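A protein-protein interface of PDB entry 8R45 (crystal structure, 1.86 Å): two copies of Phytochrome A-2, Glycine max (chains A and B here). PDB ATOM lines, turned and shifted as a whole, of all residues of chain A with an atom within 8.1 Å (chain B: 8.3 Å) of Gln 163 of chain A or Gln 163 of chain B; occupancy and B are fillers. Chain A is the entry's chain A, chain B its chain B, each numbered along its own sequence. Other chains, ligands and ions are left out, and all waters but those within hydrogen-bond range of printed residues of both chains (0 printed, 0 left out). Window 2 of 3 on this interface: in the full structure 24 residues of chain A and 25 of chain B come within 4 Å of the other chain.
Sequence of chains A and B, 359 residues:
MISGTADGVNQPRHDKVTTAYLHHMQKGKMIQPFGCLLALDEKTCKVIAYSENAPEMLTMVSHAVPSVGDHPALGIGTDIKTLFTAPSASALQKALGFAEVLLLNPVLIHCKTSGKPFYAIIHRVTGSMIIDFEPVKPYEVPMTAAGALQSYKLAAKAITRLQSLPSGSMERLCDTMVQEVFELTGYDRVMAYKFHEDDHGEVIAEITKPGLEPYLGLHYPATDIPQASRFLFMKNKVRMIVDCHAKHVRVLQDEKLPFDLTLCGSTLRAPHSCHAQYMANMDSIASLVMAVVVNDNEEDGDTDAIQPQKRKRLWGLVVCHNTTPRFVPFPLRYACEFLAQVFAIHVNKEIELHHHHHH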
ATOM      1  N   ALA A 156       7.297 -33.191 -22.607  1.00  0.00           N
ATOM      2  CA  ALA A 156       7.291 -31.728 -22.548  1.00  0.00           C
ATOM      3  C   ALA A 156       7.986 -31.139 -23.772  1.00  0.00           C
ATOM      4  O   ALA A 156       7.497 -30.137 -24.319  1.00  0.00           O
ATOM      5  CB  ALA A 156       7.900 -31.230 -21.269  1.00  0.00           C
ATOM      6  N   LYS A 157       9.097 -31.766 -24.195  1.00  0.00           N
ATOM      7  CA  LYS A 157       9.788 -31.373 -25.423  1.00  0.00           C
ATOM      8  C   LYS A 157       8.891 -31.588 -26.647  1.00  0.00           C
ATOM      9  O   LYS A 157       8.859 -30.752 -27.540  1.00  0.00           O
ATOM     10  CB  LYS A 157      11.119 -32.115 -25.585  1.00  0.00           C
ATOM     11  CG  LYS A 157      12.172 -31.636 -24.592  1.00  0.00           C
ATOM     12  CD  LYS A 157      13.549 -32.224 -24.766  1.00  0.00           C
ATOM     13  CE  LYS A 157      14.556 -31.481 -23.917  1.00  0.00           C
ATOM     14  NZ  LYS A 157      15.930 -31.960 -24.175  1.00  0.00           N
ATOM     15  N   ALA A 158       8.193 -32.718 -26.702  1.00  0.00           N
ATOM     16  CA  ALA A 158       7.221 -32.974 -27.757  1.00  0.00           C
ATOM     17  C   ALA A 158       6.171 -31.853 -27.808  1.00  0.00           C
ATOM     18  O   ALA A 158       5.829 -31.327 -28.874  1.00  0.00           O
ATOM     19  CB  ALA A 158       6.585 -34.337 -27.542  1.00  0.00           C
ATOM     20  N   ILE A 159       5.663 -31.472 -26.648  1.00  0.00           N
ATOM     21  CA  ILE A 159       4.710 -30.383 -26.539  1.00  0.00           C
ATOM     22  C   ILE A 159       5.308 -29.078 -27.065  1.00  0.00           C
ATOM     23  O   ILE A 159       4.614 -28.354 -27.776  1.00  0.00           O
ATOM     24  CB  ILE A 159       4.235 -30.253 -25.095  1.00  0.00           C
ATOM     25  CG1 ILE A 159       3.166 -31.299 -24.802  1.00  0.00           C
ATOM     26  CG2 ILE A 159       3.793 -28.840 -24.764  1.00  0.00           C
ATOM     27  CD1 ILE A 159       2.912 -31.468 -23.319  1.00  0.00           C
ATOM     28  N   THR A 160       6.577 -28.772 -26.769  1.00  0.00           N
ATOM     29  CA  THR A 160       7.119 -27.539 -27.333  1.00  0.00           C
ATOM     30  C   THR A 160       7.198 -27.619 -28.866  1.00  0.00           C
ATOM     31  O   THR A 160       6.948 -26.620 -29.530  1.00  0.00           O
ATOM     32  CB  THR A 160       8.468 -27.113 -26.740  1.00  0.00           C
ATOM     33  OG1 THR A 160       9.460 -28.010 -27.247  1.00  0.00           O
ATOM     34  CG2 THR A 160       8.438 -27.080 -25.227  1.00  0.00           C
ATOM     35  N   ARG A 161       7.492 -28.791 -29.445  1.00  0.00           N
ATOM     36  CA  ARG A 161       7.504 -28.923 -30.895  1.00  0.00           C
ATOM     37  C   ARG A 161       6.095 -28.824 -31.482  1.00  0.00           C
ATOM     38  O   ARG A 161       5.956 -28.286 -32.582  1.00  0.00           O
ATOM     39  CB  ARG A 161       8.215 -30.188 -31.381  1.00  0.00           C
ATOM     40  CG  ARG A 161       9.715 -30.134 -31.131  1.00  0.00           C
ATOM     41  CD  ARG A 161      10.447 -31.336 -31.682  1.00  0.00           C
ATOM     42  NE  ARG A 161      10.147 -32.562 -30.947  1.00  0.00           N
ATOM     43  CZ  ARG A 161      10.773 -32.982 -29.854  1.00  0.00           C
ATOM     44  NH1 ARG A 161      10.430 -34.128 -29.312  1.00  0.00           N
ATOM     45  NH2 ARG A 161      11.783 -32.291 -29.330  1.00  0.00           N
ATOM     46  N   LEU A 162       5.065 -29.348 -30.805  1.00  0.00           N
ATOM     47  CA  LEU A 162       3.709 -29.108 -31.286  1.00  0.00           C
ATOM     48  C   LEU A 162       3.379 -27.617 -31.265  1.00  0.00           C
ATOM     49  O   LEU A 162       2.679 -27.107 -32.152  1.00  0.00           O
ATOM     50  CB  LEU A 162       2.672 -29.820 -30.427  1.00  0.00           C
ATOM     51  CG  LEU A 162       2.549 -31.320 -30.562  1.00  0.00           C
ATOM     52  CD1 LEU A 162       1.383 -31.782 -29.713  1.00  0.00           C
ATOM     53  CD2 LEU A 162       2.347 -31.725 -32.006  1.00  0.00           C
ATOM     54  N   GLN A 163       3.815 -26.923 -30.211  1.00  0.00           N
ATOM     55  CA  GLN A 163       3.575 -25.490 -30.050  1.00  0.00           C
ATOM     56  C   GLN A 163       4.237 -24.660 -31.149  1.00  0.00           C
ATOM     57  O   GLN A 163       3.653 -23.695 -31.608  1.00  0.00           O
ATOM     58  CB  GLN A 163       4.050 -24.995 -28.675  1.00  0.00           C
ATOM     59  CG  GLN A 163       3.211 -25.509 -27.501  1.00  0.00           C
ATOM     60  CD  GLN A 163       3.628 -25.091 -26.093  1.00  0.00           C
ATOM     61  OE1 GLN A 163       2.812 -25.192 -25.183  1.00  0.00           O
ATOM     62  NE2 GLN A 163       4.857 -24.618 -25.869  1.00  0.00           N
ATOM     63  N   SER A 164       5.452 -24.995 -31.577  1.00  0.00           N
ATOM     64  CA  SER A 164       6.156 -24.144 -32.516  1.00  0.00           C
ATOM     65  C   SER A 164       5.689 -24.382 -33.951  1.00  0.00           C
ATOM     66  O   SER A 164       6.120 -23.689 -34.858  1.00  0.00           O
ATOM     67  CB  SER A 164       7.638 -24.345 -32.382  1.00  0.00           C
ATOM     68  OG  SER A 164       8.006 -25.639 -32.823  1.00  0.00           O
ATOM     69  N   LEU A 165       4.861 -25.402 -34.184  1.00  0.00           N
ATOM     70  CA  LEU A 165       4.361 -25.648 -35.525  1.00  0.00           C
ATOM     71  C   LEU A 165       3.642 -24.406 -36.024  1.00  0.00           C
ATOM     72  O   LEU A 165       2.760 -23.914 -35.339  1.00  0.00           O
ATOM     73  CB  LEU A 165       3.349 -26.795 -35.508  1.00  0.00           C
ATOM     74  CG  LEU A 165       3.899 -28.194 -35.743  1.00  0.00           C
ATOM     75  CD1 LEU A 165       2.738 -29.182 -35.734  1.00  0.00           C
ATOM     76  CD2 LEU A 165       4.673 -28.275 -37.057  1.00  0.00           C
ATOM     77  N   PRO A 166       3.890 -23.950 -37.268  1.00  0.00           N
ATOM     78  CA  PRO A 166       3.000 -22.958 -37.887  1.00  0.00           C
ATOM     79  C   PRO A 166       1.553 -23.463 -37.901  1.00  0.00           C
ATOM     80  O   PRO A 166       1.332 -24.609 -38.275  1.00  0.00           O
ATOM     81  CB  PRO A 166       3.537 -22.809 -39.323  1.00  0.00           C
ATOM     82  CG  PRO A 166       4.928 -23.449 -39.324  1.00  0.00           C
ATOM     83  CD  PRO A 166       4.967 -24.413 -38.154  1.00  0.00           C
ATOM     84  N   SER A 167       0.590 -22.626 -37.479  1.00  0.00           N
ATOM     85  CA  SER A 167      -0.842 -22.889 -37.619  1.00  0.00           C
ATOM     86  C   SER A 167      -1.237 -23.109 -39.084  1.00  0.00           C
ATOM     87  O   SER A 167      -0.478 -22.803 -40.007  1.00  0.00           O
ATOM     88  CB  SER A 167      -1.658 -21.727 -37.088  1.00  0.00           C
ATOM     89  OG  SER A 167      -1.546 -21.591 -35.687  1.00  0.00           O
ATOM     90  N   LEU A 173      -0.089 -31.064 -38.246  1.00  0.00           N
ATOM     91  CA  LEU A 173      -0.270 -31.196 -36.808  1.00  0.00           C
ATOM     92  C   LEU A 173      -0.400 -32.678 -36.462  1.00  0.00           C
ATOM     93  O   LEU A 173       0.247 -33.151 -35.532  1.00  0.00           O
ATOM     94  CB  LEU A 173      -1.532 -30.436 -36.383  1.00  0.00           C
ATOM     95  CG  LEU A 173      -1.936 -30.569 -34.911  1.00  0.00           C
ATOM     96  CD1 LEU A 173      -0.861 -30.000 -33.969  1.00  0.00           C
ATOM     97  CD2 LEU A 173      -3.274 -29.896 -34.649  1.00  0.00           C
ATOM     98  N   THR A 176       2.814 -34.628 -37.017  1.00  0.00           N
ATOM     99  CA  THR A 176       3.797 -34.329 -36.005  1.00  0.00           C
ATOM    100  C   THR A 176       3.432 -35.114 -34.741  1.00  0.00           C
ATOM    101  O   THR A 176       4.289 -35.729 -34.136  1.00  0.00           O
ATOM    102  CB  THR A 176       3.929 -32.811 -35.769  1.00  0.00           C
ATOM    103  OG1 THR A 176       4.428 -32.167 -36.948  1.00  0.00           O
ATOM    104  CG2 THR A 176       4.844 -32.488 -34.602  1.00  0.00           C
ATOM    105  N   PHE A 338      -0.960 -35.862 -20.900  1.00  0.00           N
ATOM    106  CA  PHE A 338      -0.847 -34.424 -20.982  1.00  0.00           C
ATOM    107  C   PHE A 338      -0.533 -34.066 -22.428  1.00  0.00           C
ATOM    108  O   PHE A 338      -1.014 -33.046 -22.917  1.00  0.00           O
ATOM    109  CB  PHE A 338       0.207 -33.812 -20.042  1.00  0.00           C
ATOM    110  CG  PHE A 338       0.191 -32.295 -20.036  1.00  0.00           C
ATOM    111  CD1 PHE A 338      -0.987 -31.595 -19.790  1.00  0.00           C
ATOM    112  CD2 PHE A 338       1.326 -31.555 -20.348  1.00  0.00           C
ATOM    113  CE1 PHE A 338      -1.034 -30.207 -19.840  1.00  0.00           C
ATOM    114  CE2 PHE A 338       1.289 -30.174 -20.361  1.00  0.00           C
ATOM    115  CZ  PHE A 338       0.113 -29.495 -20.117  1.00  0.00           C
ATOM    116  N   VAL A 342      -2.729 -31.420 -24.795  1.00  0.00           N
ATOM    117  CA  VAL A 342      -2.205 -30.286 -25.526  1.00  0.00           C
ATOM    118  C   VAL A 342      -2.536 -30.446 -27.013  1.00  0.00           C
ATOM    119  O   VAL A 342      -2.966 -29.484 -27.673  1.00  0.00           O
ATOM    120  CB  VAL A 342      -0.697 -30.150 -25.285  1.00  0.00           C
ATOM    121  CG1 VAL A 342      -0.036 -29.197 -26.265  1.00  0.00           C
ATOM    122  CG2 VAL A 342      -0.400 -29.766 -23.842  1.00  0.00           C
ATOM    123  N   ILE A 345      -6.044 -29.390 -27.691  1.00  0.00           N
ATOM    124  CA  ILE A 345      -6.196 -27.934 -27.747  1.00  0.00           C
ATOM    125  C   ILE A 345      -5.802 -27.405 -29.127  1.00  0.00           C
ATOM    126  O   ILE A 345      -6.527 -26.572 -29.696  1.00  0.00           O
ATOM    127  CB  ILE A 345      -5.429 -27.246 -26.598  1.00  0.00           C
ATOM    128  CG1 ILE A 345      -6.245 -27.307 -25.306  1.00  0.00           C
ATOM    129  CG2 ILE A 345      -5.025 -25.809 -26.925  1.00  0.00           C
ATOM    130  CD1 ILE A 345      -5.389 -27.381 -24.054  1.00  0.00           C
ATOM    131  N   HIS A 346      -4.661 -27.869 -29.663  1.00  0.00           N
ATOM    132  CA  HIS A 346      -4.216 -27.450 -30.978  1.00  0.00           C
ATOM    133  C   HIS A 346      -5.134 -27.955 -32.093  1.00  0.00           C
ATOM    134  O   HIS A 346      -5.361 -27.258 -33.100  1.00  0.00           O
ATOM    135  CB  HIS A 346      -2.772 -27.890 -31.217  1.00  0.00           C
ATOM    136  CG  HIS A 346      -1.767 -27.041 -30.531  1.00  0.00           C
ATOM    137  ND1 HIS A 346      -1.402 -27.197 -29.211  1.00  0.00           N
ATOM    138  CD2 HIS A 346      -1.013 -26.055 -31.021  1.00  0.00           C
ATOM    139  CE1 HIS A 346      -0.466 -26.303 -28.915  1.00  0.00           C
ATOM    140  NE2 HIS A 346      -0.208 -25.610 -30.009  1.00  0.00           N
ATOM    141  N   LYS A 349      -8.070 -25.589 -32.156  1.00  0.00           N
ATOM    142  CA  LYS A 349      -7.696 -24.318 -32.759  1.00  0.00           C
ATOM    143  C   LYS A 349      -7.668 -24.431 -34.280  1.00  0.00           C
ATOM    144  O   LYS A 349      -8.103 -23.499 -34.957  1.00  0.00           O
ATOM    145  CB  LYS A 349      -6.339 -23.819 -32.259  1.00  0.00           C
ATOM    146  CG  LYS A 349      -6.426 -23.019 -30.972  1.00  0.00           C
ATOM    147  CD  LYS A 349      -5.097 -22.693 -30.320  1.00  0.00           C
ATOM    148  CE  LYS A 349      -5.305 -22.089 -28.942  1.00  0.00           C
ATOM    149  NZ  LYS A 349      -4.114 -22.228 -28.071  1.00  0.00           N
ATOM    150  N   ALA B 156       5.369 -27.971 -16.963  1.00  0.00           N
ATOM    151  CA  ALA B 156       4.858 -28.061 -18.332  1.00  0.00           C
ATOM    152  C   ALA B 156       3.629 -27.172 -18.513  1.00  0.00           C
ATOM    153  O   ALA B 156       3.492 -26.522 -19.539  1.00  0.00           O
ATOM    154  CB  ALA B 156       4.542 -29.500 -18.728  1.00  0.00           C
ATOM    155  N   LYS B 157       2.731 -27.114 -17.527  1.00  0.00           N
ATOM    156  CA  LYS B 157       1.606 -26.180 -17.613  1.00  0.00           C
ATOM    157  C   LYS B 157       2.061 -24.722 -17.627  1.00  0.00           C
ATOM    158  O   LYS B 157       1.519 -23.905 -18.388  1.00  0.00           O
ATOM    159  CB  LYS B 157       0.614 -26.398 -16.474  1.00  0.00           C
ATOM    160  CG  LYS B 157      -0.227 -27.662 -16.599  1.00  0.00           C
ATOM    161  CD  LYS B 157      -1.233 -27.748 -15.453  1.00  0.00           C
ATOM    162  CE  LYS B 157      -2.581 -28.297 -15.852  1.00  0.00           C
ATOM    163  NZ  LYS B 157      -2.420 -29.567 -16.587  1.00  0.00           N
ATOM    164  N   ALA B 158       3.074 -24.394 -16.819  1.00  0.00           N
ATOM    165  CA  ALA B 158       3.677 -23.072 -16.906  1.00  0.00           C
ATOM    166  C   ALA B 158       4.207 -22.791 -18.318  1.00  0.00           C
ATOM    167  O   ALA B 158       4.022 -21.713 -18.856  1.00  0.00           O
ATOM    168  CB  ALA B 158       4.764 -22.895 -15.865  1.00  0.00           C
ATOM    169  N   ILE B 159       4.905 -23.743 -18.917  1.00  0.00           N
ATOM    170  CA  ILE B 159       5.398 -23.595 -20.280  1.00  0.00           C
ATOM    171  C   ILE B 159       4.272 -23.334 -21.278  1.00  0.00           C
ATOM    172  O   ILE B 159       4.416 -22.450 -22.125  1.00  0.00           O
ATOM    173  CB  ILE B 159       6.234 -24.828 -20.633  1.00  0.00           C
ATOM    174  CG1 ILE B 159       7.589 -24.727 -19.946  1.00  0.00           C
ATOM    175  CG2 ILE B 159       6.327 -25.029 -22.137  1.00  0.00           C
ATOM    176  CD1 ILE B 159       8.344 -26.037 -19.929  1.00  0.00           C
ATOM    177  N   THR B 160       3.140 -24.055 -21.175  1.00  0.00           N
ATOM    178  CA  THR B 160       2.030 -23.788 -22.086  1.00  0.00           C
ATOM    179  C   THR B 160       1.507 -22.359 -21.907  1.00  0.00           C
ATOM    180  O   THR B 160       1.108 -21.750 -22.885  1.00  0.00           O
ATOM    181  CB  THR B 160       0.863 -24.788 -21.989  1.00  0.00           C
ATOM    182  OG1 THR B 160       0.150 -24.700 -20.753  1.00  0.00           O
ATOM    183  CG2 THR B 160       1.320 -26.215 -22.149  1.00  0.00           C
ATOM    184  N   ARG B 161       1.501 -21.807 -20.688  1.00  0.00           N
ATOM    185  CA  ARG B 161       1.062 -20.429 -20.491  1.00  0.00           C
ATOM    186  C   ARG B 161       2.086 -19.432 -21.053  1.00  0.00           C
ATOM    187  O   ARG B 161       1.690 -18.388 -21.577  1.00  0.00           O
ATOM    188  CB  ARG B 161       0.737 -20.202 -19.008  1.00  0.00           C
ATOM    189  CG  ARG B 161      -0.599 -20.823 -18.598  1.00  0.00           C
ATOM    190  CD  ARG B 161      -1.059 -20.549 -17.172  1.00  0.00           C
ATOM    191  NE  ARG B 161      -0.073 -21.008 -16.204  1.00  0.00           N
ATOM    192  CZ  ARG B 161      -0.114 -22.185 -15.600  1.00  0.00           C
ATOM    193  NH1 ARG B 161       0.801 -22.527 -14.703  1.00  0.00           N
ATOM    194  NH2 ARG B 161      -1.104 -23.009 -15.888  1.00  0.00           N
ATOM    195  N   LEU B 162       3.391 -19.723 -20.976  1.00  0.00           N
ATOM    196  CA  LEU B 162       4.368 -18.856 -21.628  1.00  0.00           C
ATOM    197  C   LEU B 162       4.142 -18.819 -23.139  1.00  0.00           C
ATOM    198  O   LEU B 162       4.312 -17.776 -23.771  1.00  0.00           O
ATOM    199  CB  LEU B 162       5.798 -19.327 -21.384  1.00  0.00           C
ATOM    200  CG  LEU B 162       6.360 -19.094 -19.995  1.00  0.00           C
ATOM    201  CD1 LEU B 162       7.796 -19.572 -19.946  1.00  0.00           C
ATOM    202  CD2 LEU B 162       6.286 -17.619 -19.578  1.00  0.00           C
ATOM    203  N   GLN B 163       3.866 -19.985 -23.730  1.00  0.00           N
ATOM    204  CA  GLN B 163       3.717 -20.095 -25.174  1.00  0.00           C
ATOM    205  C   GLN B 163       2.492 -19.331 -25.656  1.00  0.00           C
ATOM    206  O   GLN B 163       2.484 -18.831 -26.762  1.00  0.00           O
ATOM    207  CB  GLN B 163       3.595 -21.561 -25.606  1.00  0.00           C
ATOM    208  CG  GLN B 163       2.808 -21.768 -26.911  1.00  0.00           C
ATOM    209  CD  GLN B 163       3.526 -21.379 -28.187  1.00  0.00           C
ATOM    210  OE1 GLN B 163       4.659 -20.892 -28.193  1.00  0.00           O
ATOM    211  NE2 GLN B 163       2.864 -21.626 -29.304  1.00  0.00           N
ATOM    212  N   SER B 164       1.413 -19.326 -24.889  1.00  0.00           N
ATOM    213  CA  SER B 164       0.189 -18.723 -25.372  1.00  0.00           C
ATOM    214  C   SER B 164       0.155 -17.218 -25.086  1.00  0.00           C
ATOM    215  O   SER B 164      -0.794 -16.551 -25.503  1.00  0.00           O
ATOM    216  CB  SER B 164      -0.992 -19.428 -24.790  1.00  0.00           C
ATOM    217  OG  SER B 164      -1.156 -19.040 -23.444  1.00  0.00           O
ATOM    218  N   LEU B 165       1.187 -16.660 -24.420  1.00  0.00           N
ATOM    219  CA  LEU B 165       1.309 -15.207 -24.295  1.00  0.00           C
ATOM    220  C   LEU B 165       1.383 -14.547 -25.666  1.00  0.00           C
ATOM    221  O   LEU B 165       2.301 -14.861 -26.412  1.00  0.00           O
ATOM    222  CB  LEU B 165       2.628 -14.850 -23.600  1.00  0.00           C
ATOM    223  CG  LEU B 165       2.612 -14.633 -22.100  1.00  0.00           C
ATOM    224  CD1 LEU B 165       3.892 -13.906 -21.730  1.00  0.00           C
ATOM    225  CD2 LEU B 165       1.385 -13.852 -21.646  1.00  0.00           C
ATOM    226  N   PRO B 166       0.564 -13.519 -25.999  1.00  0.00           N
ATOM    227  CA  PRO B 166       0.793 -12.748 -27.234  1.00  0.00           C
ATOM    228  C   PRO B 166       2.224 -12.207 -27.317  1.00  0.00           C
ATOM    229  O   PRO B 166       2.776 -11.769 -26.311  1.00  0.00           O
ATOM    230  CB  PRO B 166      -0.231 -11.601 -27.172  1.00  0.00           C
ATOM    231  CG  PRO B 166      -0.847 -11.651 -25.775  1.00  0.00           C
ATOM    232  CD  PRO B 166      -0.583 -13.036 -25.215  1.00  0.00           C
ATOM    233  N   SER B 167       2.863 -12.290 -28.487  1.00  0.00           N
ATOM    234  CA  SER B 167       4.223 -11.787 -28.668  1.00  0.00           C
ATOM    235  C   SER B 167       4.287 -10.268 -28.489  1.00  0.00           C
ATOM    236  O   SER B 167       3.262  -9.619 -28.324  1.00  0.00           O
ATOM    237  CB  SER B 167       4.722 -12.132 -30.032  1.00  0.00           C
ATOM    238  OG  SER B 167       4.326 -13.446 -30.357  1.00  0.00           O
ATOM    239  N   LEU B 173       6.350 -10.958 -20.889  1.00  0.00           N
ATOM    240  CA  LEU B 173       6.993 -12.266 -20.852  1.00  0.00           C
ATOM    241  C   LEU B 173       7.690 -12.478 -19.502  1.00  0.00           C
ATOM    242  O   LEU B 173       7.449 -13.488 -18.825  1.00  0.00           O
ATOM    243  CB  LEU B 173       7.978 -12.404 -22.018  1.00  0.00           C
ATOM    244  CG  LEU B 173       8.807 -13.695 -22.047  1.00  0.00           C
ATOM    245  CD1 LEU B 173       7.922 -14.934 -22.159  1.00  0.00           C
ATOM    246  CD2 LEU B 173       9.836 -13.687 -23.171  1.00  0.00           C
ATOM    247  N   THR B 176       5.273 -12.789 -16.568  1.00  0.00           N
ATOM    248  CA  THR B 176       4.623 -14.085 -16.501  1.00  0.00           C
ATOM    249  C   THR B 176       5.579 -15.127 -15.921  1.00  0.00           C
ATOM    250  O   THR B 176       5.188 -15.955 -15.111  1.00  0.00           O
ATOM    251  CB  THR B 176       4.198 -14.574 -17.891  1.00  0.00           C
ATOM    252  OG1 THR B 176       3.368 -13.541 -18.418  1.00  0.00           O
ATOM    253  CG2 THR B 176       3.500 -15.919 -17.808  1.00  0.00           C
ATOM    254  N   PHE B 338      14.022 -26.918 -17.118  1.00  0.00           N
ATOM    255  CA  PHE B 338      13.432 -26.952 -18.439  1.00  0.00           C
ATOM    256  C   PHE B 338      12.572 -25.694 -18.653  1.00  0.00           C
ATOM    257  O   PHE B 338      12.605 -25.136 -19.734  1.00  0.00           O
ATOM    258  CB  PHE B 338      12.685 -28.278 -18.689  1.00  0.00           C
ATOM    259  CG  PHE B 338      12.199 -28.365 -20.113  1.00  0.00           C
ATOM    260  CD1 PHE B 338      13.097 -28.289 -21.167  1.00  0.00           C
ATOM    261  CD2 PHE B 338      10.850 -28.348 -20.390  1.00  0.00           C
ATOM    262  CE1 PHE B 338      12.664 -28.263 -22.485  1.00  0.00           C
ATOM    263  CE2 PHE B 338      10.402 -28.377 -21.700  1.00  0.00           C
ATOM    264  CZ  PHE B 338      11.308 -28.353 -22.748  1.00  0.00           C
ATOM    265  N   VAL B 342      12.959 -22.997 -21.815  1.00  0.00           N
ATOM    266  CA  VAL B 342      11.885 -22.552 -22.668  1.00  0.00           C
ATOM    267  C   VAL B 342      11.782 -21.030 -22.612  1.00  0.00           C
ATOM    268  O   VAL B 342      11.540 -20.359 -23.620  1.00  0.00           O
ATOM    269  CB  VAL B 342      10.561 -23.242 -22.285  1.00  0.00           C
ATOM    270  CG1 VAL B 342       9.362 -22.586 -22.950  1.00  0.00           C
ATOM    271  CG2 VAL B 342      10.625 -24.722 -22.639  1.00  0.00           C
ATOM    272  N   ILE B 345      14.261 -19.352 -24.793  1.00  0.00           N
ATOM    273  CA  ILE B 345      13.876 -19.365 -26.194  1.00  0.00           C
ATOM    274  C   ILE B 345      12.915 -18.216 -26.475  1.00  0.00           C
ATOM    275  O   ILE B 345      13.060 -17.548 -27.499  1.00  0.00           O
ATOM    276  CB  ILE B 345      13.295 -20.737 -26.600  1.00  0.00           C
ATOM    277  CG1 ILE B 345      14.427 -21.761 -26.723  1.00  0.00           C
ATOM    278  CG2 ILE B 345      12.453 -20.662 -27.876  1.00  0.00           C
ATOM    279  CD1 ILE B 345      13.959 -23.207 -26.667  1.00  0.00           C
ATOM    280  N   HIS B 346      11.916 -18.023 -25.611  1.00  0.00           N
ATOM    281  CA  HIS B 346      10.970 -16.929 -25.797  1.00  0.00           C
ATOM    282  C   HIS B 346      11.613 -15.557 -25.627  1.00  0.00           C
ATOM    283  O   HIS B 346      11.204 -14.635 -26.320  1.00  0.00           O
ATOM    284  CB  HIS B 346       9.745 -17.039 -24.896  1.00  0.00           C
ATOM    285  CG  HIS B 346       8.846 -18.100 -25.397  1.00  0.00           C
ATOM    286  ND1 HIS B 346       8.990 -19.427 -25.027  1.00  0.00           N
ATOM    287  CD2 HIS B 346       7.793 -18.045 -26.210  1.00  0.00           C
ATOM    288  CE1 HIS B 346       8.063 -20.154 -25.645  1.00  0.00           C
ATOM    289  NE2 HIS B 346       7.316 -19.336 -26.362  1.00  0.00           N
ATOM    290  N   LYS B 349      13.297 -14.797 -28.880  1.00  0.00           N
ATOM    291  CA  LYS B 349      12.292 -14.420 -29.867  1.00  0.00           C
ATOM    292  C   LYS B 349      11.875 -12.966 -29.678  1.00  0.00           C
ATOM    293  O   LYS B 349      11.728 -12.241 -30.656  1.00  0.00           O
ATOM    294  CB  LYS B 349      10.995 -15.231 -29.780  1.00  0.00           C
ATOM    295  CG  LYS B 349      11.019 -16.620 -30.408  1.00  0.00           C
ATOM    296  CD  LYS B 349       9.782 -17.465 -30.065  1.00  0.00           C
ATOM    297  CE  LYS B 349       8.460 -16.830 -30.455  1.00  0.00           C
ATOM    298  NZ  LYS B 349       7.396 -17.075 -29.447  1.00  0.00           N
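O of Gln 163 of chain A is in hydrogen-bond range of NE2 of Gln 163 of chain B, at 3.2 Å.
O of Lys 157 of chain B sits at hydrogen-bond distance from OG1 of Thr 160 of chain B (2.8 Å). The backbone carbonyl oxygen of Lys 157 of chain A lies within hydrogen-bond range of the side-chain hydroxyl of Thr 160 of chain A, 2.8 Å away.
Phe 338 of chain B touches Ala 156 of chain A. Lys 157 of chain A touches Phe 338 of chain B (CG to CZ, 3.9 Å). CA of Thr 160 of chain B touches OE1 of Gln 163 of chain A, at 3.5 Å. Phe 338 of chain A touches Ala 156 of chain B (CE2 to CB, 3.7 Å). NZ of Lys 157 of chain B touches CE1 of Phe 338 of chain A, at 3.6 Å.
Of chain B, only Thr 160 (3.5 Å) and Gln 163 (3.2 Å) come within 4 Å of Gln 163 of chain A. Ser 164 of chain A touches none of the printed residues of chain B. Ser 167 of chain A touches none of the printed residues of chain B. Of the printed residues of chain B, Phe 338 of chain A touches Ala 156 (3.7 Å) and Lys 157 (3.6 Å). Printed residues of chain A within 4 Å of Lys 157 of chain B: Phe 338. Leu 162 of chain B touches none of the printed residues of chain A. Gln 163 of chain B touches just one residue of chain A: Gln 163 (3.2 Å). Of the printed residues of chain A, Phe 338 of chain B touches Ala 156 and Lys 157. The nearest residue of chain B that does not touch Gln 163 of chain A is Ile 159 of chain B (4.03 Å).
Of the 19 printed residues of chain B, 5 touch a printed residue of chain A. Printed residues of chain A that touch a printed residue of chain B: Ala 156, Lys 157, Gln 163 and Phe 338. Hydrophobic or aromatic side chains of chain A within 4 Å of the printed part of chain B: Ala 156 and Phe 338.
Ala 156 of chain A touches Phe 338 of chain B, and with the chains exchanged Phe 338 of chain A touches Ala 156 of chain B. Lys 157 of chain A touches Phe 338 of chain B, and with the chains exchanged Phe 338 of chain A touches Lys 157 of chain B. Gln 163 of chain A touches Thr 160 of chain B, but with the chains exchanged Thr 160 of chain A does not touch Gln 163 of chain B (6.3 Å). Gln 163 of chain B touches its own counterpart, Gln 163 of chain A. 19 positions are printed for both chains. Of the 6 pairs that touch across the chains among the printed residues, 5 have their exchanged pair printed and touching as well.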
